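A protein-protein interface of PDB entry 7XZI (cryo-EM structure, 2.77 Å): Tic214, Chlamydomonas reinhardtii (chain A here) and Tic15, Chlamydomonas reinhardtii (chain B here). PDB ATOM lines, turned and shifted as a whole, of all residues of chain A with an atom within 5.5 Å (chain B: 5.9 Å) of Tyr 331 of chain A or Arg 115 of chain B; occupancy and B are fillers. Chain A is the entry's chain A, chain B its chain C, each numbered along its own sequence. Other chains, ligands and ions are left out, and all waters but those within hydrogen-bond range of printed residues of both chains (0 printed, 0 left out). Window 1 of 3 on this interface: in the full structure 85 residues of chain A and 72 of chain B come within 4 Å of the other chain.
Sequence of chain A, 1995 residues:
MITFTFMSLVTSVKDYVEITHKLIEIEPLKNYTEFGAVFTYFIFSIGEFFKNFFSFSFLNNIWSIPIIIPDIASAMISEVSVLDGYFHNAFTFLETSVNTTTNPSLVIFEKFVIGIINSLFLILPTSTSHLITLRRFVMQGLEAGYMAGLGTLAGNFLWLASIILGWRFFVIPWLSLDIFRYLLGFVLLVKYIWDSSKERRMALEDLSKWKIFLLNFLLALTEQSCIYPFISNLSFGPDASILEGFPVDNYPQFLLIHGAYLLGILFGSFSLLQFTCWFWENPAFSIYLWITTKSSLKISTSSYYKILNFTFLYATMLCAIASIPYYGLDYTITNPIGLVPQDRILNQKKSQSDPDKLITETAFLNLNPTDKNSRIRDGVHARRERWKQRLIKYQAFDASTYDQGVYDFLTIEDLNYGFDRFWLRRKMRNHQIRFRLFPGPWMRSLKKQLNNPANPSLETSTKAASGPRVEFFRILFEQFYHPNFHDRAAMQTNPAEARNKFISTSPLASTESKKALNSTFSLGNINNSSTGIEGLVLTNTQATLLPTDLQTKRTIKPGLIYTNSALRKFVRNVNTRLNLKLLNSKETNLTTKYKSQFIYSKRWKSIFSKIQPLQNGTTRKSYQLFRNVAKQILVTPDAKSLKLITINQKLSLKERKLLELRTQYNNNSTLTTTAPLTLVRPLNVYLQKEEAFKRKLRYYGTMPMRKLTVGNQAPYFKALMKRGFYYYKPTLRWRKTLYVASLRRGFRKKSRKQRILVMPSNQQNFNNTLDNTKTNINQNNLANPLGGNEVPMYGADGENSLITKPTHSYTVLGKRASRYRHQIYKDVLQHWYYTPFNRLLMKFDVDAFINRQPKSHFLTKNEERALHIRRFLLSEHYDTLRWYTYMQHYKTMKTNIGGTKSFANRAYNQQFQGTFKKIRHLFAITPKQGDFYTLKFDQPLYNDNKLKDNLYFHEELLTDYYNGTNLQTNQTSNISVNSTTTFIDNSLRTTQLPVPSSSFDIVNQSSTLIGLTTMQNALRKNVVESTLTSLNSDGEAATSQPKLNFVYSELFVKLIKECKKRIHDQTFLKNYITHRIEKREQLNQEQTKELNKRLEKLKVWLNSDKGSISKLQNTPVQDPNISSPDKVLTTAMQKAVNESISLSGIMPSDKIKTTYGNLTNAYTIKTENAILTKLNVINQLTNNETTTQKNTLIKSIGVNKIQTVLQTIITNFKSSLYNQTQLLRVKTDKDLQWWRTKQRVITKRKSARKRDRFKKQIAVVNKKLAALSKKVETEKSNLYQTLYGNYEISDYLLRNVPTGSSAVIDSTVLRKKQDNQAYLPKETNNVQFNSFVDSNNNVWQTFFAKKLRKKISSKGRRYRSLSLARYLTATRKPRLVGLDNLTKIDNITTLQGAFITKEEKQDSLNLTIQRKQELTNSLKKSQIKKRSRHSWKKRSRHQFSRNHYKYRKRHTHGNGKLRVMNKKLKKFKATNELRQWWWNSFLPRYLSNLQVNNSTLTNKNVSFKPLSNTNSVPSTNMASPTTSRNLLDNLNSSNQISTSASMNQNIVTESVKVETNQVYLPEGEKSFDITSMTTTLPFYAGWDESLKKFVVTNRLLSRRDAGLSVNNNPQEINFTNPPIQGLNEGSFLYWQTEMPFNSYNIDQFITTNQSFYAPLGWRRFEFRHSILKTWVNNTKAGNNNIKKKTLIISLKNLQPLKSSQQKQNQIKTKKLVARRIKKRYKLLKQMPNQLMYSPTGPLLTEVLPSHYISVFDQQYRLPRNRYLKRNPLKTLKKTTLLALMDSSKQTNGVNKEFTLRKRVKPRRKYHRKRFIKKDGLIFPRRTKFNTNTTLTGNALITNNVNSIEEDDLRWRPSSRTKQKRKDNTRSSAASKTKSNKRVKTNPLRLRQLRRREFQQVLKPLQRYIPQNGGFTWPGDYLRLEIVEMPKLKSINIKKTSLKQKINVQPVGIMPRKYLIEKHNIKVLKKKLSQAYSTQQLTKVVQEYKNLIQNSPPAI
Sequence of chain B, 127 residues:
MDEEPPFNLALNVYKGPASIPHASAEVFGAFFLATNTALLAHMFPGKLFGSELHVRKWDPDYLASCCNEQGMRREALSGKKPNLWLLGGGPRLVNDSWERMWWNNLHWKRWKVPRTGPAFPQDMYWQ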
ATOM      1  N   ASP A 178     -13.887  23.457   6.332  1.00  0.00           N
ATOM      2  CA  ASP A 178     -12.957  22.770   7.224  1.00  0.00           C
ATOM      3  C   ASP A 178     -11.532  23.300   7.083  1.00  0.00           C
ATOM      4  O   ASP A 178     -10.876  23.611   8.083  1.00  0.00           O
ATOM      5  CB  ASP A 178     -13.000  21.265   6.953  1.00  0.00           C
ATOM      6  CG  ASP A 178     -12.447  20.451   8.104  1.00  0.00           C
ATOM      7  OD1 ASP A 178     -12.055  21.055   9.124  1.00  0.00           O
ATOM      8  OD2 ASP A 178     -12.407  19.207   7.993  1.00  0.00           O
ATOM      9  N   ILE A 179     -11.033  23.412   5.851  1.00  0.00           N
ATOM     10  CA  ILE A 179      -9.627  23.745   5.635  1.00  0.00           C
ATOM     11  C   ILE A 179      -9.387  25.246   5.496  1.00  0.00           C
ATOM     12  O   ILE A 179      -8.272  25.718   5.769  1.00  0.00           O
ATOM     13  CB  ILE A 179      -9.088  23.004   4.397  1.00  0.00           C
ATOM     14  CG1 ILE A 179      -9.560  21.550   4.399  1.00  0.00           C
ATOM     15  CG2 ILE A 179      -7.569  23.047   4.355  1.00  0.00           C
ATOM     16  CD1 ILE A 179      -9.067  20.747   5.582  1.00  0.00           C
ATOM     17  N   TYR A 182      -8.377  26.673   8.813  1.00  0.00           N
ATOM     18  CA  TYR A 182      -6.992  26.383   9.172  1.00  0.00           C
ATOM     19  C   TYR A 182      -6.033  27.278   8.398  1.00  0.00           C
ATOM     20  O   TYR A 182      -5.074  27.817   8.969  1.00  0.00           O
ATOM     21  CB  TYR A 182      -6.663  24.914   8.903  1.00  0.00           C
ATOM     22  CG  TYR A 182      -7.607  23.905   9.522  1.00  0.00           C
ATOM     23  CD1 TYR A 182      -8.342  24.203  10.660  1.00  0.00           C
ATOM     24  CD2 TYR A 182      -7.755  22.642   8.962  1.00  0.00           C
ATOM     25  CE1 TYR A 182      -9.199  23.275  11.221  1.00  0.00           C
ATOM     26  CE2 TYR A 182      -8.608  21.710   9.515  1.00  0.00           C
ATOM     27  CZ  TYR A 182      -9.328  22.031  10.643  1.00  0.00           C
ATOM     28  OH  TYR A 182     -10.181  21.104  11.199  1.00  0.00           O
ATOM     29  N   TYR A 326      -0.530  16.475  13.414  1.00  0.00           N
ATOM     30  CA  TYR A 326      -1.785  15.915  13.905  1.00  0.00           C
ATOM     31  C   TYR A 326      -2.577  15.247  12.787  1.00  0.00           C
ATOM     32  O   TYR A 326      -3.104  14.142  12.961  1.00  0.00           O
ATOM     33  CB  TYR A 326      -2.613  17.013  14.572  1.00  0.00           C
ATOM     34  CG  TYR A 326      -3.495  16.528  15.700  1.00  0.00           C
ATOM     35  CD1 TYR A 326      -2.965  16.265  16.955  1.00  0.00           C
ATOM     36  CD2 TYR A 326      -4.859  16.349  15.514  1.00  0.00           C
ATOM     37  CE1 TYR A 326      -3.764  15.830  17.990  1.00  0.00           C
ATOM     38  CE2 TYR A 326      -5.667  15.912  16.546  1.00  0.00           C
ATOM     39  CZ  TYR A 326      -5.114  15.656  17.782  1.00  0.00           C
ATOM     40  OH  TYR A 326      -5.911  15.221  18.813  1.00  0.00           O
ATOM     41  N   TYR A 327      -2.673  15.898  11.632  1.00  0.00           N
ATOM     42  CA  TYR A 327      -3.492  15.420  10.527  1.00  0.00           C
ATOM     43  C   TYR A 327      -2.617  14.956   9.370  1.00  0.00           C
ATOM     44  O   TYR A 327      -1.597  15.580   9.060  1.00  0.00           O
ATOM     45  CB  TYR A 327      -4.444  16.513  10.035  1.00  0.00           C
ATOM     46  CG  TYR A 327      -5.260  17.158  11.127  1.00  0.00           C
ATOM     47  CD1 TYR A 327      -6.410  16.552  11.610  1.00  0.00           C
ATOM     48  CD2 TYR A 327      -4.885  18.377  11.671  1.00  0.00           C
ATOM     49  CE1 TYR A 327      -7.161  17.139  12.607  1.00  0.00           C
ATOM     50  CE2 TYR A 327      -5.630  18.973  12.669  1.00  0.00           C
ATOM     51  CZ  TYR A 327      -6.767  18.349  13.132  1.00  0.00           C
ATOM     52  OH  TYR A 327      -7.513  18.939  14.125  1.00  0.00           O
ATOM     53  N   GLY A 328      -3.026  13.857   8.735  1.00  0.00           N
ATOM     54  CA  GLY A 328      -2.358  13.392   7.539  1.00  0.00           C
ATOM     55  C   GLY A 328      -2.816  14.133   6.295  1.00  0.00           C
ATOM     56  O   GLY A 328      -3.732  14.953   6.322  1.00  0.00           O
ATOM     57  N   LEU A 329      -2.148  13.831   5.178  1.00  0.00           N
ATOM     58  CA  LEU A 329      -2.471  14.488   3.916  1.00  0.00           C
ATOM     59  C   LEU A 329      -3.797  14.023   3.334  1.00  0.00           C
ATOM     60  O   LEU A 329      -4.380  14.739   2.513  1.00  0.00           O
ATOM     61  CB  LEU A 329      -1.354  14.262   2.895  1.00  0.00           C
ATOM     62  CG  LEU A 329      -0.108  15.135   3.041  1.00  0.00           C
ATOM     63  CD1 LEU A 329       0.775  15.030   1.808  1.00  0.00           C
ATOM     64  CD2 LEU A 329      -0.510  16.578   3.291  1.00  0.00           C
ATOM     65  N   ASP A 330      -4.282  12.844   3.727  1.00  0.00           N
ATOM     66  CA  ASP A 330      -5.559  12.367   3.206  1.00  0.00           C
ATOM     67  C   ASP A 330      -6.711  13.239   3.689  1.00  0.00           C
ATOM     68  O   ASP A 330      -7.684  13.453   2.958  1.00  0.00           O
ATOM     69  CB  ASP A 330      -5.779  10.907   3.607  1.00  0.00           C
ATOM     70  CG  ASP A 330      -5.728  10.698   5.109  1.00  0.00           C
ATOM     71  OD1 ASP A 330      -4.972  11.421   5.789  1.00  0.00           O
ATOM     72  OD2 ASP A 330      -6.447   9.808   5.609  1.00  0.00           O
ATOM     73  N   TYR A 331      -6.619  13.747   4.919  1.00  0.00           N
ATOM     74  CA  TYR A 331      -7.674  14.590   5.466  1.00  0.00           C
ATOM     75  C   TYR A 331      -7.514  16.053   5.067  1.00  0.00           C
ATOM     76  O   TYR A 331      -8.504  16.791   5.031  1.00  0.00           O
ATOM     77  CB  TYR A 331      -7.706  14.452   6.989  1.00  0.00           C
ATOM     78  CG  TYR A 331      -8.577  15.466   7.691  1.00  0.00           C
ATOM     79  CD1 TYR A 331      -9.961  15.392   7.618  1.00  0.00           C
ATOM     80  CD2 TYR A 331      -8.016  16.491   8.436  1.00  0.00           C
ATOM     81  CE1 TYR A 331     -10.758  16.316   8.262  1.00  0.00           C
ATOM     82  CE2 TYR A 331      -8.804  17.418   9.082  1.00  0.00           C
ATOM     83  CZ  TYR A 331     -10.174  17.326   8.992  1.00  0.00           C
ATOM     84  OH  TYR A 331     -10.962  18.249   9.635  1.00  0.00           O
ATOM     85  N   THR A 332      -6.293  16.490   4.764  1.00  0.00           N
ATOM     86  CA  THR A 332      -6.051  17.894   4.453  1.00  0.00           C
ATOM     87  C   THR A 332      -6.033  18.190   2.958  1.00  0.00           C
ATOM     88  O   THR A 332      -6.305  19.329   2.563  1.00  0.00           O
ATOM     89  CB  THR A 332      -4.727  18.352   5.072  1.00  0.00           C
ATOM     90  OG1 THR A 332      -3.679  17.460   4.679  1.00  0.00           O
ATOM     91  CG2 THR A 332      -4.824  18.375   6.589  1.00  0.00           C
ATOM     92  N   ILE A 333      -5.722  17.206   2.121  1.00  0.00           N
ATOM     93  CA  ILE A 333      -5.596  17.405   0.681  1.00  0.00           C
ATOM     94  C   ILE A 333      -6.730  16.727  -0.080  1.00  0.00           C
ATOM     95  O   ILE A 333      -7.425  17.365  -0.871  1.00  0.00           O
ATOM     96  CB  ILE A 333      -4.219  16.919   0.173  1.00  0.00           C
ATOM     97  CG1 ILE A 333      -3.097  17.750   0.795  1.00  0.00           C
ATOM     98  CG2 ILE A 333      -4.158  16.986  -1.344  1.00  0.00           C
ATOM     99  CD1 ILE A 333      -3.202  19.231   0.508  1.00  0.00           C
ATOM    100  N   THR A 334      -6.929  15.426   0.142  1.00  0.00           N
ATOM    101  CA  THR A 334      -7.937  14.693  -0.615  1.00  0.00           C
ATOM    102  C   THR A 334      -9.356  15.011  -0.158  1.00  0.00           C
ATOM    103  O   THR A 334     -10.291  14.936  -0.964  1.00  0.00           O
ATOM    104  CB  THR A 334      -7.689  13.187  -0.514  1.00  0.00           C
ATOM    105  OG1 THR A 334      -7.869  12.761   0.840  1.00  0.00           O
ATOM    106  CG2 THR A 334      -6.276  12.848  -0.961  1.00  0.00           C
ATOM    107  N   ASN A 335      -9.542  15.353   1.118  1.00  0.00           N
ATOM    108  CA  ASN A 335     -10.883  15.667   1.612  1.00  0.00           C
ATOM    109  C   ASN A 335     -11.506  16.872   0.916  1.00  0.00           C
ATOM    110  O   ASN A 335     -12.657  16.759   0.460  1.00  0.00           O
ATOM    111  CB  ASN A 335     -10.842  15.854   3.133  1.00  0.00           C
ATOM    112  CG  ASN A 335     -12.160  16.348   3.699  1.00  0.00           C
ATOM    113  OD1 ASN A 335     -13.234  15.952   3.246  1.00  0.00           O
ATOM    114  ND2 ASN A 335     -12.084  17.224   4.693  1.00  0.00           N
ATOM    115  N   PRO A 336     -10.843  18.032   0.797  1.00  0.00           N
ATOM    116  CA  PRO A 336     -11.472  19.145   0.069  1.00  0.00           C
ATOM    117  C   PRO A 336     -11.696  18.862  -1.406  1.00  0.00           C
ATOM    118  O   PRO A 336     -12.562  19.502  -2.013  1.00  0.00           O
ATOM    119  CB  PRO A 336     -10.488  20.305   0.272  1.00  0.00           C
ATOM    120  CG  PRO A 336      -9.195  19.656   0.556  1.00  0.00           C
ATOM    121  CD  PRO A 336      -9.528  18.424   1.336  1.00  0.00           C
ATOM    122  N   ARG B  56      -7.305  21.807  19.144  1.00  0.00           N
ATOM    123  CA  ARG B  56      -8.521  22.603  19.179  1.00  0.00           C
ATOM    124  C   ARG B  56      -9.053  22.662  20.603  1.00  0.00           C
ATOM    125  O   ARG B  56      -8.533  22.017  21.517  1.00  0.00           O
ATOM    126  CB  ARG B  56      -9.592  22.033  18.238  1.00  0.00           C
ATOM    127  CG  ARG B  56     -10.062  20.638  18.612  1.00  0.00           C
ATOM    128  CD  ARG B  56     -11.238  20.203  17.754  1.00  0.00           C
ATOM    129  NE  ARG B  56     -10.886  20.124  16.344  1.00  0.00           N
ATOM    130  CZ  ARG B  56     -10.453  19.023  15.740  1.00  0.00           C
ATOM    131  NH1 ARG B  56     -10.313  17.884  16.398  1.00  0.00           N
ATOM    132  NH2 ARG B  56     -10.154  19.068  14.446  1.00  0.00           N
ATOM    133  N   ASP B  59     -14.753  20.214  19.760  1.00  0.00           N
ATOM    134  CA  ASP B  59     -14.960  19.497  18.511  1.00  0.00           C
ATOM    135  C   ASP B  59     -16.064  20.172  17.700  1.00  0.00           C
ATOM    136  O   ASP B  59     -17.056  20.639  18.268  1.00  0.00           O
ATOM    137  CB  ASP B  59     -15.327  18.039  18.790  1.00  0.00           C
ATOM    138  CG  ASP B  59     -15.252  17.171  17.551  1.00  0.00           C
ATOM    139  OD1 ASP B  59     -14.138  16.988  17.018  1.00  0.00           O
ATOM    140  OD2 ASP B  59     -16.308  16.669  17.110  1.00  0.00           O
ATOM    141  N   PRO B  60     -15.917  20.252  16.374  1.00  0.00           N
ATOM    142  CA  PRO B  60     -16.970  20.886  15.561  1.00  0.00           C
ATOM    143  C   PRO B  60     -18.322  20.203  15.680  1.00  0.00           C
ATOM    144  O   PRO B  60     -19.359  20.880  15.639  1.00  0.00           O
ATOM    145  CB  PRO B  60     -16.408  20.792  14.135  1.00  0.00           C
ATOM    146  CG  PRO B  60     -14.933  20.693  14.318  1.00  0.00           C
ATOM    147  CD  PRO B  60     -14.733  19.902  15.573  1.00  0.00           C
ATOM    148  N   ASP B  61     -18.340  18.876  15.824  1.00  0.00           N
ATOM    149  CA  ASP B  61     -19.605  18.164  15.976  1.00  0.00           C
ATOM    150  C   ASP B  61     -20.308  18.556  17.270  1.00  0.00           C
ATOM    151  O   ASP B  61     -21.535  18.688  17.298  1.00  0.00           O
ATOM    152  CB  ASP B  61     -19.367  16.656  15.930  1.00  0.00           C
ATOM    153  CG  ASP B  61     -18.712  16.206  14.638  1.00  0.00           C
ATOM    154  OD1 ASP B  61     -17.492  16.422  14.481  1.00  0.00           O
ATOM    155  OD2 ASP B  61     -19.418  15.638  13.779  1.00  0.00           O
ATOM    156  N   HIS B 107     -20.616  12.604   3.224  1.00  0.00           N
ATOM    157  CA  HIS B 107     -19.207  12.928   3.036  1.00  0.00           C
ATOM    158  C   HIS B 107     -18.631  13.604   4.271  1.00  0.00           C
ATOM    159  O   HIS B 107     -17.499  13.317   4.676  1.00  0.00           O
ATOM    160  CB  HIS B 107     -19.036  13.820   1.807  1.00  0.00           C
ATOM    161  CG  HIS B 107     -17.640  14.324   1.613  1.00  0.00           C
ATOM    162  ND1 HIS B 107     -16.599  13.505   1.230  1.00  0.00           N
ATOM    163  CD2 HIS B 107     -17.112  15.562   1.753  1.00  0.00           C
ATOM    164  CE1 HIS B 107     -15.492  14.217   1.141  1.00  0.00           C
ATOM    165  NE2 HIS B 107     -15.775  15.468   1.454  1.00  0.00           N
ATOM    166  N   TRP B 108     -19.395  14.515   4.878  1.00  0.00           N
ATOM    167  CA  TRP B 108     -18.936  15.147   6.112  1.00  0.00           C
ATOM    168  C   TRP B 108     -18.800  14.130   7.240  1.00  0.00           C
ATOM    169  O   TRP B 108     -17.820  14.155   7.994  1.00  0.00           O
ATOM    170  CB  TRP B 108     -19.885  16.273   6.520  1.00  0.00           C
ATOM    171  CG  TRP B 108     -19.624  16.786   7.904  1.00  0.00           C
ATOM    172  CD1 TRP B 108     -20.216  16.365   9.058  1.00  0.00           C
ATOM    173  CD2 TRP B 108     -18.697  17.811   8.280  1.00  0.00           C
ATOM    174  NE1 TRP B 108     -19.717  17.064  10.129  1.00  0.00           N
ATOM    175  CE2 TRP B 108     -18.784  17.959   9.678  1.00  0.00           C
ATOM    176  CE3 TRP B 108     -17.804  18.619   7.571  1.00  0.00           C
ATOM    177  CZ2 TRP B 108     -18.012  18.882  10.381  1.00  0.00           C
ATOM    178  CZ3 TRP B 108     -17.039  19.534   8.270  1.00  0.00           C
ATOM    179  CH2 TRP B 108     -17.147  19.659   9.661  1.00  0.00           C
ATOM    180  N   LYS B 109     -19.776  13.230   7.375  1.00  0.00           N
ATOM    181  CA  LYS B 109     -19.780  12.305   8.505  1.00  0.00           C
ATOM    182  C   LYS B 109     -18.748  11.196   8.348  1.00  0.00           C
ATOM    183  O   LYS B 109     -18.287  10.639   9.349  1.00  0.00           O
ATOM    184  CB  LYS B 109     -21.174  11.709   8.690  1.00  0.00           C
ATOM    185  CG  LYS B 109     -22.199  12.696   9.213  1.00  0.00           C
ATOM    186  CD  LYS B 109     -23.523  12.015   9.493  1.00  0.00           C
ATOM    187  CE  LYS B 109     -24.498  12.969  10.159  1.00  0.00           C
ATOM    188  NZ  LYS B 109     -25.785  12.301  10.494  1.00  0.00           N
ATOM    189  N   TRP B 111     -15.722  11.390   7.566  1.00  0.00           N
ATOM    190  CA  TRP B 111     -14.401  11.816   8.005  1.00  0.00           C
ATOM    191  C   TRP B 111     -14.329  12.028   9.512  1.00  0.00           C
ATOM    192  O   TRP B 111     -13.513  12.829   9.978  1.00  0.00           O
ATOM    193  CB  TRP B 111     -13.987  13.098   7.281  1.00  0.00           C
ATOM    194  CG  TRP B 111     -13.613  12.897   5.849  1.00  0.00           C
ATOM    195  CD1 TRP B 111     -14.396  13.124   4.756  1.00  0.00           C
ATOM    196  CD2 TRP B 111     -12.353  12.435   5.350  1.00  0.00           C
ATOM    197  NE1 TRP B 111     -13.704  12.828   3.607  1.00  0.00           N
ATOM    198  CE2 TRP B 111     -12.446  12.404   3.946  1.00  0.00           C
ATOM    199  CE3 TRP B 111     -11.156  12.043   5.957  1.00  0.00           C
ATOM    200  CZ2 TRP B 111     -11.389  11.995   3.137  1.00  0.00           C
ATOM    201  CZ3 TRP B 111     -10.108  11.638   5.153  1.00  0.00           C
ATOM    202  CH2 TRP B 111     -10.231  11.617   3.758  1.00  0.00           C
ATOM    203  N   LYS B 112     -15.166  11.331  10.284  1.00  0.00           N
ATOM    204  CA  LYS B 112     -15.238  11.592  11.718  1.00  0.00           C
ATOM    205  C   LYS B 112     -13.941  11.212  12.424  1.00  0.00           C
ATOM    206  O   LYS B 112     -13.387  12.006  13.191  1.00  0.00           O
ATOM    207  CB  LYS B 112     -16.420  10.841  12.330  1.00  0.00           C
ATOM    208  CG  LYS B 112     -16.630  11.123  13.809  1.00  0.00           C
ATOM    209  CD  LYS B 112     -16.918  12.595  14.055  1.00  0.00           C
ATOM    210  CE  LYS B 112     -17.261  12.856  15.511  1.00  0.00           C
ATOM    211  NZ  LYS B 112     -16.165  12.429  16.422  1.00  0.00           N
ATOM    212  N   VAL B 113     -13.448  10.001  12.186  1.00  0.00           N
ATOM    213  CA  VAL B 113     -12.240   9.517  12.853  1.00  0.00           C
ATOM    214  C   VAL B 113     -11.014  10.337  12.455  1.00  0.00           C
ATOM    215  O   VAL B 113     -10.276  10.784  13.346  1.00  0.00           O
ATOM    216  CB  VAL B 113     -12.022   8.019  12.584  1.00  0.00           C
ATOM    217  CG1 VAL B 113     -10.747   7.543  13.257  1.00  0.00           C
ATOM    218  CG2 VAL B 113     -13.218   7.218  13.071  1.00  0.00           C
ATOM    219  N   PRO B 114     -10.731  10.561  11.162  1.00  0.00           N
ATOM    220  CA  PRO B 114      -9.547  11.368  10.824  1.00  0.00           C
ATOM    221  C   PRO B 114      -9.619  12.799  11.327  1.00  0.00           C
ATOM    222  O   PRO B 114      -8.580  13.376  11.671  1.00  0.00           O
ATOM    223  CB  PRO B 114      -9.509  11.315   9.289  1.00  0.00           C
ATOM    224  CG  PRO B 114     -10.311  10.126   8.925  1.00  0.00           C
ATOM    225  CD  PRO B 114     -11.397  10.065   9.942  1.00  0.00           C
ATOM    226  N   ARG B 115     -10.814  13.392  11.375  1.00  0.00           N
ATOM    227  CA  ARG B 115     -10.933  14.791  11.774  1.00  0.00           C
ATOM    228  C   ARG B 115     -10.584  14.988  13.244  1.00  0.00           C
ATOM    229  O   ARG B 115      -9.959  15.989  13.611  1.00  0.00           O
ATOM    230  CB  ARG B 115     -12.346  15.300  11.481  1.00  0.00           C
ATOM    231  CG  ARG B 115     -12.610  16.724  11.939  1.00  0.00           C
ATOM    232  CD  ARG B 115     -13.908  17.282  11.364  1.00  0.00           C
ATOM    233  NE  ARG B 115     -15.069  16.471  11.703  1.00  0.00           N
ATOM    234  CZ  ARG B 115     -15.714  15.687  10.845  1.00  0.00           C
ATOM    235  NH1 ARG B 115     -15.344  15.599   9.579  1.00  0.00           N
ATOM    236  NH2 ARG B 115     -16.755  14.979  11.270  1.00  0.00           N
ATOM    237  N   THR B 116     -10.974  14.046  14.100  1.00  0.00           N
ATOM    238  CA  THR B 116     -10.798  14.205  15.541  1.00  0.00           C
ATOM    239  C   THR B 116      -9.489  13.589  16.033  1.00  0.00           C
ATOM    240  O   THR B 116      -8.640  14.288  16.596  1.00  0.00           O
ATOM    241  CB  THR B 116     -11.992  13.591  16.279  1.00  0.00           C
ATOM    242  OG1 THR B 116     -11.989  12.172  16.095  1.00  0.00           O
ATOM    243  CG2 THR B 116     -13.293  14.156  15.736  1.00  0.00           C
ATOM    244  N   GLY B 117      -9.313  12.287  15.824  1.00  0.00           N
ATOM    245  CA  GLY B 117      -8.184  11.570  16.368  1.00  0.00           C
ATOM    246  C   GLY B 117      -6.858  11.943  15.737  1.00  0.00           C
ATOM    247  O   GLY B 117      -6.781  12.326  14.564  1.00  0.00           O
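OD1 of Asn 335 of chain A lies within hydrogen-bond range of NE2 of His 107 of chain B (3.1 Å).
The side-chain amide oxygen (OD1) of Asn 335 of chain A is in hydrogen-bond range of the indole nitrogen (NE1) of Trp 111 of chain B (3.2 Å).
The side-chain hydroxyl of Tyr 327 of chain A sits at hydrogen-bond distance from the guanidinium group of Arg 56 of chain B, 2.7 Å away.
The guanidinium group (NH2) of Arg 56 of chain B sits at hydrogen-bond distance from the backbone carbonyl oxygen (O) of Arg 115 of chain B.
The backbone carbonyl oxygen (O) of Trp 111 of chain B lies close to the guanidinium group (NH1) of Arg 115 of chain B.
O of Lys 112 of chain B sits at hydrogen-bond distance from OG1 of Thr 116 of chain B (3.2 Å).
The backbone NH (N) of Asn 335 of chain A lies within hydrogen-bond range of the backbone carbonyl oxygen (O) of Asp 330 of chain A (3.2 Å).
The guanidinium group of Arg 56 of chain B is in salt-bridge range of the side-chain carboxylate of Asp 59 of chain B, at 3.98 Å.
OD1 of Asp 178 of chain A sits at hydrogen-bond distance from OH of Tyr 182 of chain A (2.8 Å).
Among the printed residues, pairs that only touch across the chains: Tyr 327 of chain A with Arg 115 of chain B, Tyr 331 of chain A with Arg 115 of chain B, Asp 330 of chain A with Trp 111 of chain B, Tyr 326 of chain A with Thr 116 of chain B, Tyr 182 of chain A with Arg 56 of chain B, Tyr 331 of chain A with Trp 111 of chain B, Tyr 327 of chain A with Pro 114 of chain B and Thr 334 of chain A with Trp 111 of chain B.
Of the printed residues of chain B, Tyr 327 of chain A touches Arg 56, Pro 114 and Arg 115.
Tyr 331 of chain A touches just these residues of chain B: Trp 111 (3.8 Å) and Arg 115 (3.2 Å).
Thr 332 of chain A touches none of the printed residues of chain B.
Of the printed residues of chain B, Thr 334 of chain A touches Trp 111.
Printed residues of chain A within 4 Å of Arg 56 of chain B: Tyr 182 and Tyr 327.
Val 113 of chain B touches none of the printed residues of chain A.
Of the printed residues of chain A, Pro 114 of chain B touches Tyr 327 (3.8 Å).
Of chain A, only Tyr 327 and Tyr 331 come within 4 Å of Arg 115 of chain B.
Of the printed residues of chain A, Thr 116 of chain B touches Tyr 326.
The nearest residue of chain A that does not touch Arg 115 of chain B is Asp 178 of chain A (4.2 Å).
Of the 14 printed residues of chain A, 7 touch a printed residue of chain B.
Printed residues of chain A that touch a printed residue of chain B: Tyr 182, Tyr 326, Tyr 327, Asp 330, Tyr 331, Thr 334 and Asn 335.
Of the 14 printed residues of chain B, 6 touch a printed residue of chain A.
Printed residues of chain B that touch a printed residue of chain A: Arg 56, His 107, Trp 111, Pro 114, Arg 115 and Thr 116.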
